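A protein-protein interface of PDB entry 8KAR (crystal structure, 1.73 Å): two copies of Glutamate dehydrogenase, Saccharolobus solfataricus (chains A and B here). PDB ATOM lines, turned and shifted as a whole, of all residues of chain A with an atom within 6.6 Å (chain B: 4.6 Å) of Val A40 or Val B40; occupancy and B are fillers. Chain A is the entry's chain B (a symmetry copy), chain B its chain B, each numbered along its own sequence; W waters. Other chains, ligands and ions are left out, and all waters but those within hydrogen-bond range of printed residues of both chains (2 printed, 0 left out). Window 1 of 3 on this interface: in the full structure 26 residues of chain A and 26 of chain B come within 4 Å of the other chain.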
ATOM      1  N   PRO A  37      32.832   4.207   4.245  1.00  0.00           N
ATOM      2  CA  PRO A  37      33.253   3.165   3.324  1.00  0.00           C
ATOM      3  C   PRO A  37      34.367   3.621   2.403  1.00  0.00           C
ATOM      4  O   PRO A  37      34.378   4.786   1.979  1.00  0.00           O
ATOM      5  CB  PRO A  37      31.958   2.910   2.527  1.00  0.00           C
ATOM      6  CG  PRO A  37      31.189   4.191   2.577  1.00  0.00           C
ATOM      7  CD  PRO A  37      31.534   4.816   3.909  1.00  0.00           C
ATOM      8  N   GLU A  38      35.226   2.668   1.992  1.00  0.00           N
ATOM      9  CA  GLU A  38      36.240   2.965   1.010  1.00  0.00           C
ATOM     10  C   GLU A  38      35.682   3.337  -0.344  1.00  0.00           C
ATOM     11  O   GLU A  38      36.098   4.304  -0.936  1.00  0.00           O
ATOM     12  CB  GLU A  38      37.204   1.754   0.891  1.00  0.00           C
ATOM     13  CG  GLU A  38      37.910   1.404   2.186  1.00  0.00           C
ATOM     14  CD  GLU A  38      38.590   0.052   2.171  1.00  0.00           C
ATOM     15  OE1 GLU A  38      38.602  -0.608   1.112  1.00  0.00           O
ATOM     16  OE2 GLU A  38      39.103  -0.345   3.232  1.00  0.00           O
ATOM     17  N   ARG A  39      34.716   2.543  -0.824  1.00  0.00           N
ATOM     18  CA  ARG A  39      34.100   2.828  -2.091  1.00  0.00           C
ATOM     19  C   ARG A  39      32.592   2.481  -2.116  1.00  0.00           C
ATOM     20  O   ARG A  39      32.180   1.477  -1.595  1.00  0.00           O
ATOM     21  CB  ARG A  39      34.747   2.034  -3.259  1.00  0.00           C
ATOM     22  CG  ARG A  39      34.195   2.328  -4.632  1.00  0.00           C
ATOM     23  CD  ARG A  39      34.904   1.441  -5.648  1.00  0.00           C
ATOM     24  NE  ARG A  39      36.338   1.687  -5.615  1.00  0.00           N
ATOM     25  CZ  ARG A  39      37.233   0.896  -5.041  1.00  0.00           C
ATOM     26  NH1 ARG A  39      36.870  -0.224  -4.439  1.00  0.00           N
ATOM     27  NH2 ARG A  39      38.501   1.239  -5.068  1.00  0.00           N
ATOM     28  N   VAL A  40      31.821   3.347  -2.721  1.00  0.00           N
ATOM     29  CA  VAL A  40      30.386   3.065  -2.876  1.00  0.00           C
ATOM     30  C   VAL A  40      30.007   3.381  -4.305  1.00  0.00           C
ATOM     31  O   VAL A  40      30.334   4.424  -4.807  1.00  0.00           O
ATOM     32  CB  VAL A  40      29.500   3.889  -1.893  1.00  0.00           C
ATOM     33  CG1 VAL A  40      28.038   3.526  -2.115  1.00  0.00           C
ATOM     34  CG2 VAL A  40      29.883   3.607  -0.453  1.00  0.00           C
ATOM     35  N   MET A  41      29.358   2.416  -4.968  1.00  0.00           N
ATOM     36  CA  MET A  41      28.910   2.669  -6.304  1.00  0.00           C
ATOM     37  C   MET A  41      27.402   2.719  -6.313  1.00  0.00           C
ATOM     38  O   MET A  41      26.754   1.819  -5.760  1.00  0.00           O
ATOM     39  CB  MET A  41      29.300   1.577  -7.310  1.00  0.00           C
ATOM     40  CG  MET A  41      30.766   1.514  -7.500  1.00  0.00           C
ATOM     41  SD  MET A  41      31.405   0.085  -8.384  1.00  0.00           S
ATOM     42  CE  MET A  41      31.247  -1.184  -7.109  1.00  0.00           C
ATOM     43  N   GLN A  42      26.908   3.712  -7.023  1.00  0.00           N
ATOM     44  CA  GLN A  42      25.481   3.794  -7.332  1.00  0.00           C
ATOM     45  C   GLN A  42      25.313   3.642  -8.831  1.00  0.00           C
ATOM     46  O   GLN A  42      25.902   4.397  -9.586  1.00  0.00           O
ATOM     47  CB  GLN A  42      24.849   5.123  -6.917  1.00  0.00           C
ATOM     48  CG  GLN A  42      23.378   5.256  -7.267  1.00  0.00           C
ATOM     49  CD  GLN A  42      22.757   6.580  -6.891  1.00  0.00           C
ATOM     50  OE1 GLN A  42      22.542   6.847  -5.721  1.00  0.00           O
ATOM     51  NE2 GLN A  42      22.575   7.451  -7.869  1.00  0.00           N
ATOM     52  N   VAL A  43      24.374   2.807  -9.259  1.00  0.00           N
ATOM     53  CA  VAL A  43      24.136   2.556 -10.669  1.00  0.00           C
ATOM     54  C   VAL A  43      22.648   2.699 -11.005  1.00  0.00           C
ATOM     55  O   VAL A  43      21.777   2.433 -10.181  1.00  0.00           O
ATOM     56  CB  VAL A  43      24.676   1.189 -11.090  1.00  0.00           C
ATOM     57  CG1 VAL A  43      26.185   1.167 -10.869  1.00  0.00           C
ATOM     58  CG2 VAL A  43      24.008   0.029 -10.341  1.00  0.00           C
ATOM     59  N   TRP A  60      22.879  -0.092  -5.501  1.00  0.00           N
ATOM     60  CA  TRP A  60      24.176   0.267  -4.910  1.00  0.00           C
ATOM     61  C   TRP A  60      25.103  -0.880  -4.552  1.00  0.00           C
ATOM     62  O   TRP A  60      24.655  -1.962  -4.244  1.00  0.00           O
ATOM     63  CB  TRP A  60      23.940   1.025  -3.584  1.00  0.00           C
ATOM     64  CG  TRP A  60      23.170   2.303  -3.719  1.00  0.00           C
ATOM     65  CD1 TRP A  60      23.674   3.538  -3.975  1.00  0.00           C
ATOM     66  CD2 TRP A  60      21.747   2.466  -3.613  1.00  0.00           C
ATOM     67  NE1 TRP A  60      22.655   4.463  -4.042  1.00  0.00           N
ATOM     68  CE2 TRP A  60      21.465   3.821  -3.833  1.00  0.00           C
ATOM     69  CE3 TRP A  60      20.689   1.590  -3.368  1.00  0.00           C
ATOM     70  CZ2 TRP A  60      20.165   4.328  -3.796  1.00  0.00           C
ATOM     71  CZ3 TRP A  60      19.404   2.093  -3.343  1.00  0.00           C
ATOM     72  CH2 TRP A  60      19.157   3.445  -3.554  1.00  0.00           C
ATOM     73  N   ARG A  61      26.398  -0.565  -4.494  1.00  0.00           N
ATOM     74  CA  ARG A  61      27.376  -1.551  -4.011  1.00  0.00           C
ATOM     75  C   ARG A  61      28.259  -0.756  -3.050  1.00  0.00           C
ATOM     76  O   ARG A  61      28.876   0.206  -3.448  1.00  0.00           O
ATOM     77  CB  ARG A  61      28.253  -2.250  -5.076  1.00  0.00           C
ATOM     78  CG  ARG A  61      29.075  -3.418  -4.534  1.00  0.00           C
ATOM     79  CD  ARG A  61      28.262  -4.584  -3.988  1.00  0.00           C
ATOM     80  NE  ARG A  61      29.125  -5.595  -3.376  1.00  0.00           N
ATOM     81  CZ  ARG A  61      28.697  -6.629  -2.659  1.00  0.00           C
ATOM     82  NH1 ARG A  61      27.409  -6.821  -2.452  1.00  0.00           N
ATOM     83  NH2 ARG A  61      29.560  -7.480  -2.135  1.00  0.00           N
ATOM     84  N   SER A  62      28.217  -1.164  -1.800  1.00  0.00           N
ATOM     85  CA  SER A  62      29.028  -0.491  -0.779  1.00  0.00           C
ATOM     86  C   SER A  62      30.166  -1.413  -0.398  1.00  0.00           C
ATOM     87  O   SER A  62      29.944  -2.564   0.047  1.00  0.00           O
ATOM     88  CB  SER A  62      28.241  -0.033   0.450  1.00  0.00           C
ATOM     89  OG  SER A  62      29.076   0.479   1.539  1.00  0.00           O
ATOM     90  N   GLN A  63      31.384  -0.883  -0.551  1.00  0.00           N
ATOM     91  CA  GLN A  63      32.594  -1.656  -0.324  1.00  0.00           C
ATOM     92  C   GLN A  63      33.189  -0.915   0.843  1.00  0.00           C
ATOM     93  O   GLN A  63      33.821   0.091   0.665  1.00  0.00           O
ATOM     94  CB  GLN A  63      33.429  -1.549  -1.553  1.00  0.00           C
ATOM     95  CG  GLN A  63      32.678  -2.133  -2.751  1.00  0.00           C
ATOM     96  CD  GLN A  63      33.517  -2.266  -4.005  1.00  0.00           C
ATOM     97  OE1 GLN A  63      34.268  -1.370  -4.355  1.00  0.00           O
ATOM     98  NE2 GLN A  63      33.343  -3.384  -4.718  1.00  0.00           N
ATOM     99  N   HIS A  64      32.966  -1.458   2.007  1.00  0.00           N
ATOM    100  CA  HIS A  64      33.256  -0.674   3.211  1.00  0.00           C
ATOM    101  C   HIS A  64      34.685  -0.695   3.685  1.00  0.00           C
ATOM    102  O   HIS A  64      35.258   0.339   3.925  1.00  0.00           O
ATOM    103  CB  HIS A  64      32.386  -1.185   4.350  1.00  0.00           C
ATOM    104  CG  HIS A  64      32.731  -0.563   5.670  1.00  0.00           C
ATOM    105  ND1 HIS A  64      32.989  -1.301   6.805  1.00  0.00           N
ATOM    106  CD2 HIS A  64      32.904   0.732   6.021  1.00  0.00           C
ATOM    107  CE1 HIS A  64      33.292  -0.486   7.799  1.00  0.00           C
ATOM    108  NE2 HIS A  64      33.247   0.753   7.351  1.00  0.00           N
ATOM    109  N   GLN A  83      20.700   4.005  -0.207  1.00  0.00           N
ATOM    110  CA  GLN A  83      22.143   4.044  -0.152  1.00  0.00           C
ATOM    111  C   GLN A  83      22.639   3.834   1.280  1.00  0.00           C
ATOM    112  O   GLN A  83      23.559   3.054   1.543  1.00  0.00           O
ATOM    113  CB  GLN A  83      22.660   5.383  -0.662  1.00  0.00           C
ATOM    114  CG  GLN A  83      24.138   5.531  -0.441  1.00  0.00           C
ATOM    115  CD  GLN A  83      24.621   6.928  -0.706  1.00  0.00           C
ATOM    116  OE1 GLN A  83      24.707   7.392  -1.836  1.00  0.00           O
ATOM    117  NE2 GLN A  83      24.878   7.646   0.383  1.00  0.00           N
ATOM    118  N   VAL A  86      22.433   0.311   2.612  1.00  0.00           N
ATOM    119  CA  VAL A  86      23.380  -0.609   1.985  1.00  0.00           C
ATOM    120  C   VAL A  86      24.765  -0.414   2.608  1.00  0.00           C
ATOM    121  O   VAL A  86      25.408  -1.382   2.970  1.00  0.00           O
ATOM    122  CB  VAL A  86      23.399  -0.474   0.454  1.00  0.00           C
ATOM    123  CG1 VAL A  86      24.498  -1.326  -0.157  1.00  0.00           C
ATOM    124  CG2 VAL A  86      22.074  -0.873  -0.156  1.00  0.00           C
ATOM    125  N   ILE A  87      25.185   0.843   2.795  1.00  0.00           N
ATOM    126  CA  ILE A  87      26.410   1.166   3.518  1.00  0.00           C
ATOM    127  C   ILE A  87      26.417   0.565   4.923  1.00  0.00           C
ATOM    128  O   ILE A  87      27.394  -0.057   5.347  1.00  0.00           O
ATOM    129  CB  ILE A  87      26.685   2.676   3.553  1.00  0.00           C
ATOM    130  CG1 ILE A  87      26.769   3.275   2.158  1.00  0.00           C
ATOM    131  CG2 ILE A  87      28.000   2.880   4.303  1.00  0.00           C
ATOM    132  CD1 ILE A  87      26.819   4.784   2.086  1.00  0.00           C
ATOM    133  N   SER A  90      26.958  -3.052   4.947  1.00  0.00           N
ATOM    134  CA  SER A  90      28.313  -3.411   4.581  1.00  0.00           C
ATOM    135  C   SER A  90      29.233  -3.270   5.788  1.00  0.00           C
ATOM    136  O   SER A  90      30.181  -4.047   5.913  1.00  0.00           O
ATOM    137  CB  SER A  90      28.774  -2.639   3.338  1.00  0.00           C
ATOM    138  OG  SER A  90      29.005  -1.262   3.562  1.00  0.00           O
ATOM    139  N   PRO B  37      22.205   9.474 -13.114  1.00  0.00           N
ATOM    140  CA  PRO B  37      23.482   9.065 -13.673  1.00  0.00           C
ATOM    141  C   PRO B  37      23.593   7.561 -13.820  1.00  0.00           C
ATOM    142  O   PRO B  37      23.088   6.818 -12.965  1.00  0.00           O
ATOM    143  CB  PRO B  37      24.470   9.582 -12.608  1.00  0.00           C
ATOM    144  CG  PRO B  37      23.707   9.611 -11.323  1.00  0.00           C
ATOM    145  CD  PRO B  37      22.278   9.913 -11.710  1.00  0.00           C
ATOM    146  N   GLU B  38      24.366   7.119 -14.832  1.00  0.00           N
ATOM    147  CA  GLU B  38      24.650   5.712 -14.981  1.00  0.00           C
ATOM    148  C   GLU B  38      25.453   5.131 -13.840  1.00  0.00           C
ATOM    149  O   GLU B  38      25.120   4.092 -13.321  1.00  0.00           O
ATOM    150  CB  GLU B  38      25.375   5.479 -16.334  1.00  0.00           C
ATOM    151  CG  GLU B  38      24.569   5.914 -17.542  1.00  0.00           C
ATOM    152  CD  GLU B  38      25.374   5.997 -18.822  1.00  0.00           C
ATOM    153  OE1 GLU B  38      26.566   5.627 -18.812  1.00  0.00           O
ATOM    154  OE2 GLU B  38      24.803   6.443 -19.832  1.00  0.00           O
ATOM    155  N   ARG B  39      26.524   5.835 -13.452  1.00  0.00           N
ATOM    156  CA  ARG B  39      27.336   5.382 -12.356  1.00  0.00           C
ATOM    157  C   ARG B  39      27.889   6.546 -11.499  1.00  0.00           C
ATOM    158  O   ARG B  39      28.295   7.555 -12.014  1.00  0.00           O
ATOM    159  CB  ARG B  39      28.571   4.567 -12.829  1.00  0.00           C
ATOM    160  CG  ARG B  39      29.439   4.003 -11.731  1.00  0.00           C
ATOM    161  CD  ARG B  39      30.619   3.274 -12.362  1.00  0.00           C
ATOM    162  NE  ARG B  39      30.145   2.209 -13.231  1.00  0.00           N
ATOM    163  CZ  ARG B  39      30.110   2.264 -14.555  1.00  0.00           C
ATOM    164  NH1 ARG B  39      30.529   3.336 -15.205  1.00  0.00           N
ATOM    165  NH2 ARG B  39      29.643   1.235 -15.227  1.00  0.00           N
ATOM    166  N   VAL B  40      27.869   6.356 -10.205  1.00  0.00           N
ATOM    167  CA  VAL B  40      28.454   7.364  -9.309  1.00  0.00           C
ATOM    168  C   VAL B  40      29.312   6.639  -8.297  1.00  0.00           C
ATOM    169  O   VAL B  40      28.883   5.683  -7.706  1.00  0.00           O
ATOM    170  CB  VAL B  40      27.375   8.220  -8.579  1.00  0.00           C
ATOM    171  CG1 VAL B  40      28.068   9.241  -7.686  1.00  0.00           C
ATOM    172  CG2 VAL B  40      26.485   8.935  -9.577  1.00  0.00           C
ATOM    173  N   MET B  41      30.567   7.086  -8.162  1.00  0.00           N
ATOM    174  CA  MET B  41      31.417   6.489  -7.176  1.00  0.00           C
ATOM    175  C   MET B  41      31.686   7.499  -6.087  1.00  0.00           C
ATOM    176  O   MET B  41      32.044   8.646  -6.388  1.00  0.00           O
ATOM    177  CB  MET B  41      32.793   6.070  -7.710  1.00  0.00           C
ATOM    178  CG  MET B  41      32.680   4.977  -8.700  1.00  0.00           C
ATOM    179  SD  MET B  41      34.154   4.599  -9.658  1.00  0.00           S
ATOM    180  CE  MET B  41      34.164   5.995 -10.804  1.00  0.00           C
ATOM    181  N   GLN B  42      31.598   7.003  -4.870  1.00  0.00           N
ATOM    182  CA  GLN B  42      32.040   7.764  -3.702  1.00  0.00           C
ATOM    183  C   GLN B  42      33.226   7.045  -3.091  1.00  0.00           C
ATOM    184  O   GLN B  42      33.120   5.877  -2.757  1.00  0.00           O
ATOM    185  CB  GLN B  42      30.961   7.898  -2.626  1.00  0.00           C
ATOM    186  CG  GLN B  42      31.405   8.642  -1.381  1.00  0.00           C
ATOM    187  CD  GLN B  42      30.355   8.748  -0.300  1.00  0.00           C
ATOM    188  OE1 GLN B  42      29.395   9.485  -0.446  1.00  0.00           O
ATOM    189  NE2 GLN B  42      30.477   7.928   0.730  1.00  0.00           N
ATOM    190  N   ARG B  61      32.865  10.633  -8.059  1.00  0.00           N
ATOM    191  CA  ARG B  61      33.011  10.658  -9.521  1.00  0.00           C
ATOM    192  C   ARG B  61      31.619  10.299 -10.039  1.00  0.00           C
ATOM    193  O   ARG B  61      31.115   9.239  -9.740  1.00  0.00           O
ATOM    194  CB  ARG B  61      34.064   9.707 -10.138  1.00  0.00           C
ATOM    195  CG  ARG B  61      34.324   9.949 -11.624  1.00  0.00           C
ATOM    196  CD  ARG B  61      34.903  11.316 -11.966  1.00  0.00           C
ATOM    197  NE  ARG B  61      34.998  11.508 -13.413  1.00  0.00           N
ATOM    198  CZ  ARG B  61      35.291  12.657 -14.013  1.00  0.00           C
ATOM    199  NH1 ARG B  61      35.531  13.745 -13.307  1.00  0.00           N
ATOM    200  NH2 ARG B  61      35.338  12.729 -15.330  1.00  0.00           N
ATOM    201  N   SER B  62      31.032  11.244 -10.741  1.00  0.00           N
ATOM    202  CA  SER B  62      29.696  11.020 -11.304  1.00  0.00           C
ATOM    203  C   SER B  62      29.838  10.847 -12.801  1.00  0.00           C
ATOM    204  O   SER B  62      30.360  11.741 -13.508  1.00  0.00           O
ATOM    205  CB  SER B  62      28.676  12.107 -10.958  1.00  0.00           C
ATOM    206  OG  SER B  62      27.398  11.974 -11.661  1.00  0.00           O
ATOM    207  N   ILE B  87      27.036  15.246  -9.210  1.00  0.00           N
ATOM    208  CA  ILE B  87      26.067  14.704 -10.155  1.00  0.00           C
ATOM    209  C   ILE B  87      25.495  15.789 -11.068  1.00  0.00           C
ATOM    210  O   ILE B  87      25.433  15.628 -12.289  1.00  0.00           O
ATOM    211  CB  ILE B  87      24.951  13.913  -9.458  1.00  0.00           C
ATOM    212  CG1 ILE B  87      25.500  12.773  -8.614  1.00  0.00           C
ATOM    213  CG2 ILE B  87      24.027  13.375 -10.549  1.00  0.00           C
ATOM    214  CD1 ILE B  87      24.505  12.072  -7.718  1.00  0.00           C
HETATM  215  O   HOH W   1      32.921   6.180   0.092  1.00  0.00           O
HETATM  216  O   HOH W   2      23.739   6.113 -10.376  1.00  0.00           O
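Glu A38 touches Gln B42, and with the chains exchanged Gln A42 touches Glu B38.
Val B40 touches its own counterpart, Val A40.
Val A40 touches Met B41, and with the chains exchanged Met A41 touches Val B40.
Val A40 touches Gln B42, and with the chains exchanged Gln A42 touches Val B40.
Positions printed for both chains: 37, 38, 39, 40, 41, 42, 61, 62 and 87.
Of the 10 pairs that touch across the chains among the printed residues, 9 have their exchanged pair printed and touching as well.
Water W2 lies within hydrogen-bond range of O of Pro B37 (2.8 Å) and O of Gln A42 (2.9 Å).
Water W1 bridges the backbone carbonyl oxygen (O) of Pro A37 (2.8 Å) and the backbone carbonyl oxygen (O) of Gln B42 (2.9 Å).
Of chain B, only Val B40, Met B41 and Gln B42 come within 4 Å of Val A40.
Of the printed residues of chain B, Gln A42 touches Glu B38 (3.8 Å), Arg B39 (3.3 Å) and Val B40 (2.8 Å).
Of the printed residues of chain B, Arg A39 touches Gln B42 (3.3 Å).
Printed residues of chain A within 4 Å of Met B41: Val A40.
Of the printed residues of chain B, Met A41 touches Val B40 (3.3 Å).
Of the printed residues of chain B, Glu A38 touches Gln B42.
His A64 touches none of the printed residues of chain B.
Ser B62 touches none of the printed residues of chain A.
The nearest printed residue of chain B that does not touch Val A40 is Arg B61 (6.9 Å).
Glu A38 touches Gln B42.
Gln B42 touches Arg A39.
Val A40 touches Met B41 (O to CA, 3.3 Å).
Val B40 touches Met A41 (O to CA, 3.3 Å).
O of Gln A42 touches O of Glu B38, 3.8 Å away.
Arg B39 touches Gln A42.
CA of Val A43 touches O of Glu B38, 3.2 Å away.
The backbone NH of Val B40 sits at hydrogen-bond distance from the backbone carbonyl oxygen of Gln A42, 2.8 Å away.
The backbone carbonyl oxygen (O) of Val B40 sits close to the backbone carbonyl oxygen (O) of Val A40 (3.5 Å).
O of Gln B42 is in hydrogen-bond range of N of Val A40, at 2.8 Å.
The backbone carbonyl oxygen (O) of His A64 sits at hydrogen-bond distance from the backbone NH (N) of Glu A38.
OE1 of Gln A42 is in hydrogen-bond range of NE1 of Trp A60.
The backbone NH (N) of Glu A38 lies within hydrogen-bond range of the backbone carbonyl oxygen (O) of Gln A63 (3.2 Å).
N of Gln A63 sits at hydrogen-bond distance from O of Arg A39 (2.7 Å).
N of Arg A61 sits at hydrogen-bond distance from O of Met A41 (2.7 Å).
The backbone carbonyl oxygen (O) of Met B41 sits at hydrogen-bond distance from the backbone NH (N) of Arg B61 (2.7 Å).
Of the 16 printed residues of chain A, 6 touch a printed residue of chain B.
Printed residues of chain A that touch a printed residue of chain B: Glu A38, Arg A39, Val A40, Met A41, Gln A42 and Val A43.
Hydrophobic or aromatic side chains of chain A that line the printed part of chain B: Val A43.
Among the printed residues, 10 pairs touch across the chains.
Among the printed residues, no Asp or Glu carboxylate lies within 4 Å of a Lys or Arg side-chain nitrogen of the other chain.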
